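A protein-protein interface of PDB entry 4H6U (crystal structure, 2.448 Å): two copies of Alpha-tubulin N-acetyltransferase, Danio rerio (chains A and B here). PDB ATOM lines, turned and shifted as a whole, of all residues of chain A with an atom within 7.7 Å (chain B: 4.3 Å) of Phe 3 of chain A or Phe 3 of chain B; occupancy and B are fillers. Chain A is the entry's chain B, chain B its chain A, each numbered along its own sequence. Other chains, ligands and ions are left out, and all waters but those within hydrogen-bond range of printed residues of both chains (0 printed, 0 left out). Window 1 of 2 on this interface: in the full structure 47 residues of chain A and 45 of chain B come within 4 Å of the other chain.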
ATOM      1  N   GLY A   1       0.648  28.105  19.374  1.00  0.00           N
ATOM      2  CA  GLY A   1      -0.370  27.847  18.307  1.00  0.00           C
ATOM      3  C   GLY A   1       0.274  27.266  17.066  1.00  0.00           C
ATOM      4  O   GLY A   1       1.182  27.850  16.472  1.00  0.00           O
ATOM      5  N   SER A   2      -0.184  26.097  16.666  1.00  0.00           N
ATOM      6  CA  SER A   2       0.507  25.371  15.613  1.00  0.00           C
ATOM      7  C   SER A   2      -0.391  25.179  14.419  1.00  0.00           C
ATOM      8  O   SER A   2       0.096  25.023  13.292  1.00  0.00           O
ATOM      9  CB  SER A   2       1.017  24.019  16.126  1.00  0.00           C
ATOM     10  OG  SER A   2       2.405  24.046  16.345  1.00  0.00           O
ATOM     11  N   PHE A   3      -1.697  25.181  14.660  1.00  0.00           N
ATOM     12  CA  PHE A   3      -2.651  25.045  13.561  1.00  0.00           C
ATOM     13  C   PHE A   3      -3.657  26.218  13.508  1.00  0.00           C
ATOM     14  O   PHE A   3      -3.984  26.846  14.517  1.00  0.00           O
ATOM     15  CB  PHE A   3      -3.437  23.769  13.765  1.00  0.00           C
ATOM     16  CG  PHE A   3      -2.572  22.539  13.879  1.00  0.00           C
ATOM     17  CD1 PHE A   3      -1.929  22.014  12.778  1.00  0.00           C
ATOM     18  CD2 PHE A   3      -2.417  21.907  15.094  1.00  0.00           C
ATOM     19  CE1 PHE A   3      -1.153  20.892  12.883  1.00  0.00           C
ATOM     20  CE2 PHE A   3      -1.661  20.791  15.206  1.00  0.00           C
ATOM     21  CZ  PHE A   3      -1.019  20.271  14.104  1.00  0.00           C
ATOM     22  N   THR A   4      -4.150  26.505  12.314  1.00  0.00           N
ATOM     23  CA  THR A   4      -5.230  27.484  12.135  1.00  0.00           C
ATOM     24  C   THR A   4      -6.369  26.924  11.251  1.00  0.00           C
ATOM     25  O   THR A   4      -6.510  27.247  10.074  1.00  0.00           O
ATOM     26  CB  THR A   4      -4.704  28.797  11.549  1.00  0.00           C
ATOM     27  OG1 THR A   4      -3.981  28.505  10.356  1.00  0.00           O
ATOM     28  CG2 THR A   4      -3.777  29.514  12.548  1.00  0.00           C
ATOM     29  N   MET A   5      -7.128  26.017  11.835  1.00  0.00           N
ATOM     30  CA  MET A   5      -8.220  25.341  11.154  1.00  0.00           C
ATOM     31  C   MET A   5      -9.374  25.126  12.116  1.00  0.00           C
ATOM     32  O   MET A   5      -9.188  25.100  13.340  1.00  0.00           O
ATOM     33  CB  MET A   5      -7.745  23.982  10.630  1.00  0.00           C
ATOM     34  CG  MET A   5      -6.761  24.058   9.464  1.00  0.00           C
ATOM     35  SD  MET A   5      -6.072  22.453   8.960  1.00  0.00           S
ATOM     36  CE  MET A   5      -4.969  22.038  10.319  1.00  0.00           C
ATOM     37  N   ASP A   6     -10.582  25.072  11.568  1.00  0.00           N
ATOM     38  CA  ASP A   6     -11.745  24.633  12.328  1.00  0.00           C
ATOM     39  C   ASP A   6     -12.215  23.261  11.823  1.00  0.00           C
ATOM     40  O   ASP A   6     -12.268  23.031  10.625  1.00  0.00           O
ATOM     41  CB  ASP A   6     -12.864  25.643  12.202  1.00  0.00           C
ATOM     42  CG  ASP A   6     -12.525  26.953  12.856  1.00  0.00           C
ATOM     43  OD1 ASP A   6     -13.024  27.988  12.377  1.00  0.00           O
ATOM     44  OD2 ASP A   6     -11.765  26.943  13.852  1.00  0.00           O
ATOM     45  N   PHE A   7     -12.434  22.327  12.739  1.00  0.00           N
ATOM     46  CA  PHE A   7     -12.882  20.979  12.398  1.00  0.00           C
ATOM     47  C   PHE A   7     -14.307  20.740  12.897  1.00  0.00           C
ATOM     48  O   PHE A   7     -14.637  21.052  14.040  1.00  0.00           O
ATOM     49  CB  PHE A   7     -12.005  19.920  13.063  1.00  0.00           C
ATOM     50  CG  PHE A   7     -10.693  19.684  12.379  1.00  0.00           C
ATOM     51  CD1 PHE A   7     -10.109  20.651  11.591  1.00  0.00           C
ATOM     52  CD2 PHE A   7     -10.041  18.483  12.515  1.00  0.00           C
ATOM     53  CE1 PHE A   7      -8.885  20.426  10.981  1.00  0.00           C
ATOM     54  CE2 PHE A   7      -8.831  18.266  11.911  1.00  0.00           C
ATOM     55  CZ  PHE A   7      -8.252  19.245  11.147  1.00  0.00           C
ATOM     56  N   ILE A  19      -2.592  14.032  16.301  1.00  0.00           N
ATOM     57  CA  ILE A  19      -1.383  14.869  16.320  1.00  0.00           C
ATOM     58  C   ILE A  19      -1.328  15.862  17.475  1.00  0.00           C
ATOM     59  O   ILE A  19      -2.296  16.518  17.775  1.00  0.00           O
ATOM     60  CB  ILE A  19      -1.195  15.667  15.022  1.00  0.00           C
ATOM     61  CG1 ILE A  19      -1.336  14.742  13.804  1.00  0.00           C
ATOM     62  CG2 ILE A  19       0.171  16.285  15.034  1.00  0.00           C
ATOM     63  CD1 ILE A  19      -0.994  15.385  12.495  1.00  0.00           C
ATOM     64  N   SER A  20      -0.182  15.894  18.155  1.00  0.00           N
ATOM     65  CA  SER A  20       0.051  16.787  19.286  1.00  0.00           C
ATOM     66  C   SER A  20       1.357  17.562  19.134  1.00  0.00           C
ATOM     67  O   SER A  20       2.394  17.000  18.782  1.00  0.00           O
ATOM     68  CB  SER A  20       0.113  15.998  20.593  1.00  0.00           C
ATOM     69  OG  SER A  20      -1.126  15.399  20.866  1.00  0.00           O
ATOM     70  N   VAL A  21       1.274  18.864  19.400  1.00  0.00           N
ATOM     71  CA  VAL A  21       2.434  19.726  19.449  1.00  0.00           C
ATOM     72  C   VAL A  21       2.616  20.182  20.885  1.00  0.00           C
ATOM     73  O   VAL A  21       1.677  20.669  21.496  1.00  0.00           O
ATOM     74  CB  VAL A  21       2.254  20.968  18.530  1.00  0.00           C
ATOM     75  CG1 VAL A  21       3.516  21.837  18.503  1.00  0.00           C
ATOM     76  CG2 VAL A  21       1.867  20.524  17.122  1.00  0.00           C
ATOM     77  N   THR A  44       9.132  27.506   6.212  1.00  0.00           N
ATOM     78  CA  THR A  44       7.810  27.712   6.760  1.00  0.00           C
ATOM     79  C   THR A  44       6.823  26.794   6.082  1.00  0.00           C
ATOM     80  O   THR A  44       6.858  26.636   4.862  1.00  0.00           O
ATOM     81  CB  THR A  44       7.313  29.151   6.522  1.00  0.00           C
ATOM     82  OG1 THR A  44       8.344  30.101   6.818  1.00  0.00           O
ATOM     83  CG2 THR A  44       6.129  29.414   7.391  1.00  0.00           C
ATOM     84  N   VAL A  45       6.058  26.056   6.876  1.00  0.00           N
ATOM     85  CA  VAL A  45       4.993  25.240   6.309  1.00  0.00           C
ATOM     86  C   VAL A  45       3.651  26.026   6.467  1.00  0.00           C
ATOM     87  O   VAL A  45       3.315  26.515   7.544  1.00  0.00           O
ATOM     88  CB  VAL A  45       4.935  23.835   6.962  1.00  0.00           C
ATOM     89  CG1 VAL A  45       6.221  23.058   6.685  1.00  0.00           C
ATOM     90  CG2 VAL A  45       4.721  23.938   8.456  1.00  0.00           C
ATOM     91  N   ILE A  46       2.873  26.117   5.393  1.00  0.00           N
ATOM     92  CA  ILE A  46       1.635  26.914   5.393  1.00  0.00           C
ATOM     93  C   ILE A  46       0.431  26.008   5.179  1.00  0.00           C
ATOM     94  O   ILE A  46      -0.504  25.990   5.953  1.00  0.00           O
ATOM     95  CB  ILE A  46       1.643  27.951   4.264  1.00  0.00           C
ATOM     96  CG1 ILE A  46       2.866  28.853   4.334  1.00  0.00           C
ATOM     97  CG2 ILE A  46       0.392  28.813   4.328  1.00  0.00           C
ATOM     98  CD1 ILE A  46       2.920  29.666   5.568  1.00  0.00           C
ATOM     99  N   ASP A  47       0.433  25.305   4.062  1.00  0.00           N
ATOM    100  CA  ASP A  47      -0.655  24.399   3.741  1.00  0.00           C
ATOM    101  C   ASP A  47      -0.122  23.039   3.358  1.00  0.00           C
ATOM    102  O   ASP A  47      -0.900  22.124   3.069  1.00  0.00           O
ATOM    103  CB  ASP A  47      -1.517  24.959   2.604  1.00  0.00           C
ATOM    104  CG  ASP A  47      -2.354  26.144   3.045  1.00  0.00           C
ATOM    105  OD1 ASP A  47      -3.071  26.025   4.074  1.00  0.00           O
ATOM    106  OD2 ASP A  47      -2.289  27.184   2.361  1.00  0.00           O
ATOM    107  N   GLU A  48       1.184  22.853   3.517  1.00  0.00           N
ATOM    108  CA  GLU A  48       1.821  21.571   3.171  1.00  0.00           C
ATOM    109  C   GLU A  48       2.816  21.078   4.239  1.00  0.00           C
ATOM    110  O   GLU A  48       3.737  21.807   4.618  1.00  0.00           O
ATOM    111  CB  GLU A  48       2.564  21.724   1.830  1.00  0.00           C
ATOM    112  CG  GLU A  48       1.634  22.189   0.681  1.00  0.00           C
ATOM    113  CD  GLU A  48       0.683  21.060   0.167  1.00  0.00           C
ATOM    114  OE1 GLU A  48       0.976  19.858   0.393  1.00  0.00           O
ATOM    115  OE2 GLU A  48      -0.364  21.384  -0.436  1.00  0.00           O
ATOM    116  N   LEU A  49       2.676  19.826   4.684  1.00  0.00           N
ATOM    117  CA  LEU A  49       3.684  19.246   5.558  1.00  0.00           C
ATOM    118  C   LEU A  49       4.415  18.094   4.897  1.00  0.00           C
ATOM    119  O   LEU A  49       3.807  17.145   4.388  1.00  0.00           O
ATOM    120  CB  LEU A  49       3.064  18.698   6.837  1.00  0.00           C
ATOM    121  CG  LEU A  49       2.258  19.636   7.725  1.00  0.00           C
ATOM    122  CD1 LEU A  49       2.048  18.935   9.096  1.00  0.00           C
ATOM    123  CD2 LEU A  49       2.905  21.006   7.850  1.00  0.00           C
ATOM    124  N   GLY A  50       5.738  18.165   4.930  1.00  0.00           N
ATOM    125  CA  GLY A  50       6.546  17.073   4.456  1.00  0.00           C
ATOM    126  C   GLY A  50       7.059  17.227   3.050  1.00  0.00           C
ATOM    127  O   GLY A  50       7.617  16.296   2.518  1.00  0.00           O
ATOM    128  N   LEU A  76       1.061  11.111  16.598  1.00  0.00           N
ATOM    129  CA  LEU A  76       2.276  11.848  16.240  1.00  0.00           C
ATOM    130  C   LEU A  76       2.457  13.004  17.207  1.00  0.00           C
ATOM    131  O   LEU A  76       1.535  13.828  17.403  1.00  0.00           O
ATOM    132  CB  LEU A  76       2.140  12.370  14.813  1.00  0.00           C
ATOM    133  CG  LEU A  76       3.272  13.162  14.185  1.00  0.00           C
ATOM    134  CD1 LEU A  76       4.567  12.391  14.145  1.00  0.00           C
ATOM    135  CD2 LEU A  76       2.839  13.555  12.780  1.00  0.00           C
ATOM    136  N   LEU A  78       4.921  16.237  18.122  1.00  0.00           N
ATOM    137  CA  LEU A  78       5.899  17.202  17.605  1.00  0.00           C
ATOM    138  C   LEU A  78       6.407  18.123  18.720  1.00  0.00           C
ATOM    139  O   LEU A  78       5.603  18.680  19.495  1.00  0.00           O
ATOM    140  CB  LEU A  78       5.275  18.069  16.523  1.00  0.00           C
ATOM    141  CG  LEU A  78       4.566  17.448  15.316  1.00  0.00           C
ATOM    142  CD1 LEU A  78       4.124  18.545  14.373  1.00  0.00           C
ATOM    143  CD2 LEU A  78       5.461  16.498  14.581  1.00  0.00           C
ATOM    144  N   ARG A  88       6.781  31.895  17.301  1.00  0.00           N
ATOM    145  CA  ARG A  88       6.543  30.792  16.373  1.00  0.00           C
ATOM    146  C   ARG A  88       7.527  29.654  16.646  1.00  0.00           C
ATOM    147  O   ARG A  88       7.155  28.489  16.851  1.00  0.00           O
ATOM    148  CB  ARG A  88       6.688  31.283  14.942  1.00  0.00           C
ATOM    149  CG  ARG A  88       6.849  30.180  13.886  1.00  0.00           C
ATOM    150  CD  ARG A  88       5.516  29.618  13.440  1.00  0.00           C
ATOM    151  NE  ARG A  88       4.585  30.627  12.936  1.00  0.00           N
ATOM    152  CZ  ARG A  88       4.612  31.108  11.702  1.00  0.00           C
ATOM    153  NH1 ARG A  88       5.555  30.723  10.853  1.00  0.00           N
ATOM    154  NH2 ARG A  88       3.718  32.012  11.326  1.00  0.00           N
ATOM    155  N   SER B   2      -4.199  25.286   6.934  1.00  0.00           N
ATOM    156  CA  SER B   2      -3.250  26.335   7.351  1.00  0.00           C
ATOM    157  C   SER B   2      -2.526  25.868   8.638  1.00  0.00           C
ATOM    158  O   SER B   2      -3.138  25.382   9.597  1.00  0.00           O
ATOM    159  CB  SER B   2      -3.951  27.707   7.573  1.00  0.00           C
ATOM    160  OG  SER B   2      -3.719  28.684   6.575  1.00  0.00           O
ATOM    161  N   PHE B   3      -1.207  26.019   8.609  1.00  0.00           N
ATOM    162  CA  PHE B   3      -0.304  25.695   9.681  1.00  0.00           C
ATOM    163  C   PHE B   3       0.516  26.926  10.051  1.00  0.00           C
ATOM    164  O   PHE B   3       0.735  27.782   9.211  1.00  0.00           O
ATOM    165  CB  PHE B   3       0.671  24.618   9.234  1.00  0.00           C
ATOM    166  CG  PHE B   3       0.018  23.382   8.755  1.00  0.00           C
ATOM    167  CD1 PHE B   3      -0.588  22.530   9.654  1.00  0.00           C
ATOM    168  CD2 PHE B   3       0.018  23.061   7.404  1.00  0.00           C
ATOM    169  CE1 PHE B   3      -1.223  21.387   9.228  1.00  0.00           C
ATOM    170  CE2 PHE B   3      -0.610  21.897   6.958  1.00  0.00           C
ATOM    171  CZ  PHE B   3      -1.236  21.062   7.883  1.00  0.00           C
ATOM    172  N   THR B   4       0.980  27.000  11.298  1.00  0.00           N
ATOM    173  CA  THR B   4       1.913  28.043  11.697  1.00  0.00           C
ATOM    174  C   THR B   4       3.105  27.437  12.417  1.00  0.00           C
ATOM    175  O   THR B   4       3.288  27.612  13.616  1.00  0.00           O
ATOM    176  CB  THR B   4       1.263  29.128  12.594  1.00  0.00           C
ATOM    177  OG1 THR B   4       0.650  28.526  13.738  1.00  0.00           O
ATOM    178  CG2 THR B   4       0.221  29.937  11.803  1.00  0.00           C
ATOM    179  N   MET B   5       3.964  26.791  11.650  1.00  0.00           N
ATOM    180  CA  MET B   5       5.134  26.130  12.215  1.00  0.00           C
ATOM    181  C   MET B   5       6.313  26.336  11.254  1.00  0.00           C
ATOM    182  O   MET B   5       6.117  26.421  10.028  1.00  0.00           O
ATOM    183  CB  MET B   5       4.873  24.626  12.376  1.00  0.00           C
ATOM    184  CG  MET B   5       3.867  24.267  13.462  1.00  0.00           C
ATOM    185  SD  MET B   5       3.432  22.518  13.534  1.00  0.00           S
ATOM    186  CE  MET B   5       2.475  22.305  12.059  1.00  0.00           C
ATOM    187  N   VAL B  21      -3.318  20.681   2.520  1.00  0.00           N
ATOM    188  CA  VAL B  21      -4.580  21.386   2.654  1.00  0.00           C
ATOM    189  C   VAL B  21      -4.789  22.206   1.392  1.00  0.00           C
ATOM    190  O   VAL B  21      -3.915  22.975   0.985  1.00  0.00           O
ATOM    191  CB  VAL B  21      -4.584  22.322   3.856  1.00  0.00           C
ATOM    192  CG1 VAL B  21      -5.969  22.910   4.038  1.00  0.00           C
ATOM    193  CG2 VAL B  21      -4.171  21.572   5.110  1.00  0.00           C
ATOM    194  N   VAL B  45      -8.903  24.243  16.461  1.00  0.00           N
ATOM    195  CA  VAL B  45      -7.693  23.514  16.801  1.00  0.00           C
ATOM    196  C   VAL B  45      -6.470  24.413  16.876  1.00  0.00           C
ATOM    197  O   VAL B  45      -6.264  25.298  16.042  1.00  0.00           O
ATOM    198  CB  VAL B  45      -7.423  22.351  15.798  1.00  0.00           C
ATOM    199  CG1 VAL B  45      -8.535  21.304  15.885  1.00  0.00           C
ATOM    200  CG2 VAL B  45      -7.288  22.874  14.384  1.00  0.00           C
ATOM    201  N   ILE B  46      -5.697  24.227  17.935  1.00  0.00           N
ATOM    202  CA  ILE B  46      -4.547  25.070  18.172  1.00  0.00           C
ATOM    203  C   ILE B  46      -3.260  24.277  18.104  1.00  0.00           C
ATOM    204  O   ILE B  46      -2.419  24.530  17.231  1.00  0.00           O
ATOM    205  CB  ILE B  46      -4.630  25.687  19.549  1.00  0.00           C
ATOM    206  CG1 ILE B  46      -5.978  26.395  19.706  1.00  0.00           C
ATOM    207  CG2 ILE B  46      -3.452  26.607  19.773  1.00  0.00           C
ATOM    208  CD1 ILE B  46      -6.171  27.523  18.740  1.00  0.00           C
ATOM    209  N   ASP B  47      -3.163  23.280  18.986  1.00  0.00           N
ATOM    210  CA  ASP B  47      -2.004  22.404  19.087  1.00  0.00           C
ATOM    211  C   ASP B  47      -2.382  20.903  19.093  1.00  0.00           C
ATOM    212  O   ASP B  47      -1.529  20.053  19.333  1.00  0.00           O
ATOM    213  CB  ASP B  47      -1.210  22.749  20.345  1.00  0.00           C
ATOM    214  CG  ASP B  47      -0.464  24.090  20.233  1.00  0.00           C
ATOM    215  OD1 ASP B  47       0.285  24.308  19.249  1.00  0.00           O
ATOM    216  OD2 ASP B  47      -0.654  24.945  21.119  1.00  0.00           O
ATOM    217  N   GLU B  48      -3.655  20.585  18.853  1.00  0.00           N
ATOM    218  CA  GLU B  48      -4.152  19.186  18.819  1.00  0.00           C
ATOM    219  C   GLU B  48      -5.088  18.936  17.629  1.00  0.00           C
ATOM    220  O   GLU B  48      -6.013  19.712  17.363  1.00  0.00           O
ATOM    221  CB  GLU B  48      -4.902  18.859  20.120  1.00  0.00           C
ATOM    222  CG  GLU B  48      -4.058  19.032  21.434  1.00  0.00           C
ATOM    223  CD  GLU B  48      -3.029  17.895  21.668  1.00  0.00           C
ATOM    224  OE1 GLU B  48      -3.200  16.806  21.088  1.00  0.00           O
ATOM    225  OE2 GLU B  48      -2.016  18.098  22.365  1.00  0.00           O
ATOM    226  N   LEU B  49      -4.792  17.883  16.876  1.00  0.00           N
ATOM    227  CA  LEU B  49      -5.662  17.382  15.821  1.00  0.00           C
ATOM    228  C   LEU B  49      -6.140  15.998  16.225  1.00  0.00           C
ATOM    229  O   LEU B  49      -5.315  15.125  16.570  1.00  0.00           O
ATOM    230  CB  LEU B  49      -4.944  17.274  14.477  1.00  0.00           C
ATOM    231  CG  LEU B  49      -4.302  18.503  13.845  1.00  0.00           C
ATOM    232  CD1 LEU B  49      -3.951  18.211  12.410  1.00  0.00           C
ATOM    233  CD2 LEU B  49      -5.226  19.677  13.889  1.00  0.00           C
ATOM    234  N   ARG B  88     -10.188  31.843   9.526  1.00  0.00           N
ATOM    235  CA  ARG B  88     -10.155  30.371   9.630  1.00  0.00           C
ATOM    236  C   ARG B  88     -11.223  29.678   8.807  1.00  0.00           C
ATOM    237  O   ARG B  88     -12.417  29.876   9.030  1.00  0.00           O
ATOM    238  CB  ARG B  88     -10.352  29.948  11.082  1.00  0.00           C
ATOM    239  CG  ARG B  88      -9.100  29.734  11.875  1.00  0.00           C
ATOM    240  CD  ARG B  88      -9.438  29.768  13.360  1.00  0.00           C
ATOM    241  NE  ARG B  88      -8.280  30.124  14.171  1.00  0.00           N
ATOM    242  CZ  ARG B  88      -7.523  29.251  14.832  1.00  0.00           C
ATOM    243  NH1 ARG B  88      -7.804  27.949  14.795  1.00  0.00           N
ATOM    244  NH2 ARG B  88      -6.482  29.687  15.542  1.00  0.00           N
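Gly 1 of chain A touches Ile 46 of chain B (CA to CG2, 3.6 Å). Ser 2 of chain A touches Phe 3 of chain B (O to CA, 3.7 Å). Phe 3 of chain B touches Phe 3 of chain A (CD1 to CD1, 3.4 Å). Arg 88 of chain B touches Phe 3 of chain A (NH2 to O, 3.9 Å). Met 5 of chain A touches Ser 2 of chain B. Met 5 of chain A touches Phe 3 of chain B. Arg 88 of chain B touches Asp 6 of chain A. Phe 3 of chain B touches Glu 48 of chain A (CE2 to N, 3.997 Å). Leu 49 of chain A touches Phe 3 of chain B (CD2 to CD2, 3.6 Å). N of Met 5 of chain B touches CD of Arg 88 of chain A (3.7 Å).
Along chain A the printed residues that touch a printed residue of chain B span positions 1 to 88. Of the 11 printed residues of chain B, 11 touch a printed residue of chain A. Hydrophobic or aromatic side chains of chain B within 4 Å of the printed part of chain A: Phe 3, Met 5, Val 21, Val 45, Ile 46 and Leu 49. Among the printed residues, 40 pairs touch across the chains.
Of the printed residues of chain B, Thr 4 of chain A touches Ser 2 and Arg 88. Printed residues of chain B within 4 Å of Met 5 of chain A: Ser 2, Phe 3, Val 45 and Arg 88. Of the printed residues of chain B, Ile 19 of chain A touches Asp 47 (3.9 Å), Glu 48 (3.4 Å) and Leu 49 (2.9 Å). Printed residues of chain B within 4 Å of Arg 88 of chain A: Thr 4 (3.0 Å) and Met 5 (3.7 Å). Printed residues of chain A within 4 Å of Phe 3 of chain B: Ser 2 (3.7 Å), Phe 3 (3.4 Å), Met 5 (3.96 Å), Val 45 (3.3 Å), Ile 46 (2.7 Å), Asp 47 (3.8 Å), Glu 48 (3.997 Å) and Leu 49 (3.6 Å). Printed residues of chain A within 4 Å of Ile 46 of chain B: Gly 1 (3.6 Å), Ser 2 (2.8 Å) and Phe 3 (2.7 Å). The nearest printed residue of chain B that does not touch Phe 3 of chain A is Ser 2 of chain B (4.01 Å).
N of Ser 20 of chain A sits at hydrogen-bond distance from O of Leu 76 of chain A (2.8 Å). O of Val 45 of chain B is in hydrogen-bond range of NH1 of Arg 88 of chain B, at 3.3 Å. The backbone carbonyl oxygen of Ser 20 of chain A lies within hydrogen-bond range of the backbone NH of Leu 78 of chain A.
The backbone carbonyl oxygen (O) of Phe 3 of chain B sits close to the backbone carbonyl oxygen (O) of Val 45 of chain A (3.3 Å). The backbone carbonyl oxygen (O) of Leu 49 of chain B lies within hydrogen-bond range of the backbone NH (N) of Ile 19 of chain A. The backbone carbonyl oxygen (O) of Met 5 of chain B lies within hydrogen-bond range of the backbone NH (N) of Val 45 of chain A, at 3.2 Å. N of Ser 2 of chain B lies within hydrogen-bond range of OD1 of Asp 47 of chain A, at 3.2 Å. O of Ile 19 of chain A lies close to OE1 of Glu 48 of chain B (3.4 Å). O of Thr 4 of chain B lies close to NE of Arg 88 of chain A (3.4 Å). The backbone NH of Val 21 of chain B lies within hydrogen-bond range of the backbone carbonyl oxygen of Asp 47 of chain A (2.9 Å). The backbone carbonyl oxygen (O) of Val 45 of chain B sits close to the backbone carbonyl oxygen (O) of Phe 3 of chain A (3.1 Å). N of Ser 2 of chain A sits at hydrogen-bond distance from OD1 of Asp 47 of chain B (3.2 Å). The side-chain hydroxyl (OG) of Ser 2 of chain A lies close to the side-chain sulfur (SD) of Met 5 of chain B (3.4 Å). The backbone NH (N) of Val 21 of chain A sits at hydrogen-bond distance from the backbone carbonyl oxygen (O) of Asp 47 of chain B (3.0 Å). O of Gly 1 of chain A sits at hydrogen-bond distance from OG1 of Thr 4 of chain B. The backbone NH of Val 45 of chain B sits close to the backbone carbonyl oxygen of Met 5 of chain A (3.2 Å). OE1 of Glu 48 of chain B is in hydrogen-bond range of OG of Ser 20 of chain A, at 2.5 Å. NH1 of Arg 88 of chain B lies within hydrogen-bond range of O of Met 5 of chain A, at 3.5 Å. The backbone carbonyl oxygen of Ile 46 of chain B sits at hydrogen-bond distance from the backbone NH of Ser 2 of chain A (2.8 Å). The backbone carbonyl oxygen (O) of Ile 46 of chain A is in hydrogen-bond range of the backbone NH (N) of Phe 3 of chain B. O of Ser 2 of chain B sits at hydrogen-bond distance from N of Thr 4 of chain A (3.1 Å). The backbone NH of Thr 4 of chain B sits at hydrogen-bond distance from the backbone carbonyl oxygen of Ser 2 of chain A (2.9 Å). O of Ile 46 of chain B sits at hydrogen-bond distance from N of Phe 3 of chain A.
Ser 2 of chain A touches Asp 47 of chain B, and with the chains exchanged Asp 47 of chain A touches Ser 2 of chain B. Phe 3 of chain A touches Val 45 of chain B, and with the chains exchanged Val 45 of chain A touches Phe 3 of chain B. Val 21 of chain A touches Asp 47 of chain B, and with the chains exchanged Asp 47 of chain A touches Val 21 of chain B. Glu 48 of chain A touches Phe 3 of chain B, but with the chains exchanged Phe 3 of chain A does not touch Glu 48 of chain B (4.2 Å). 11 positions are printed for both chains. Of the 40 pairs that touch across the chains among the printed residues, 27 have their exchanged pair printed and touching as well.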
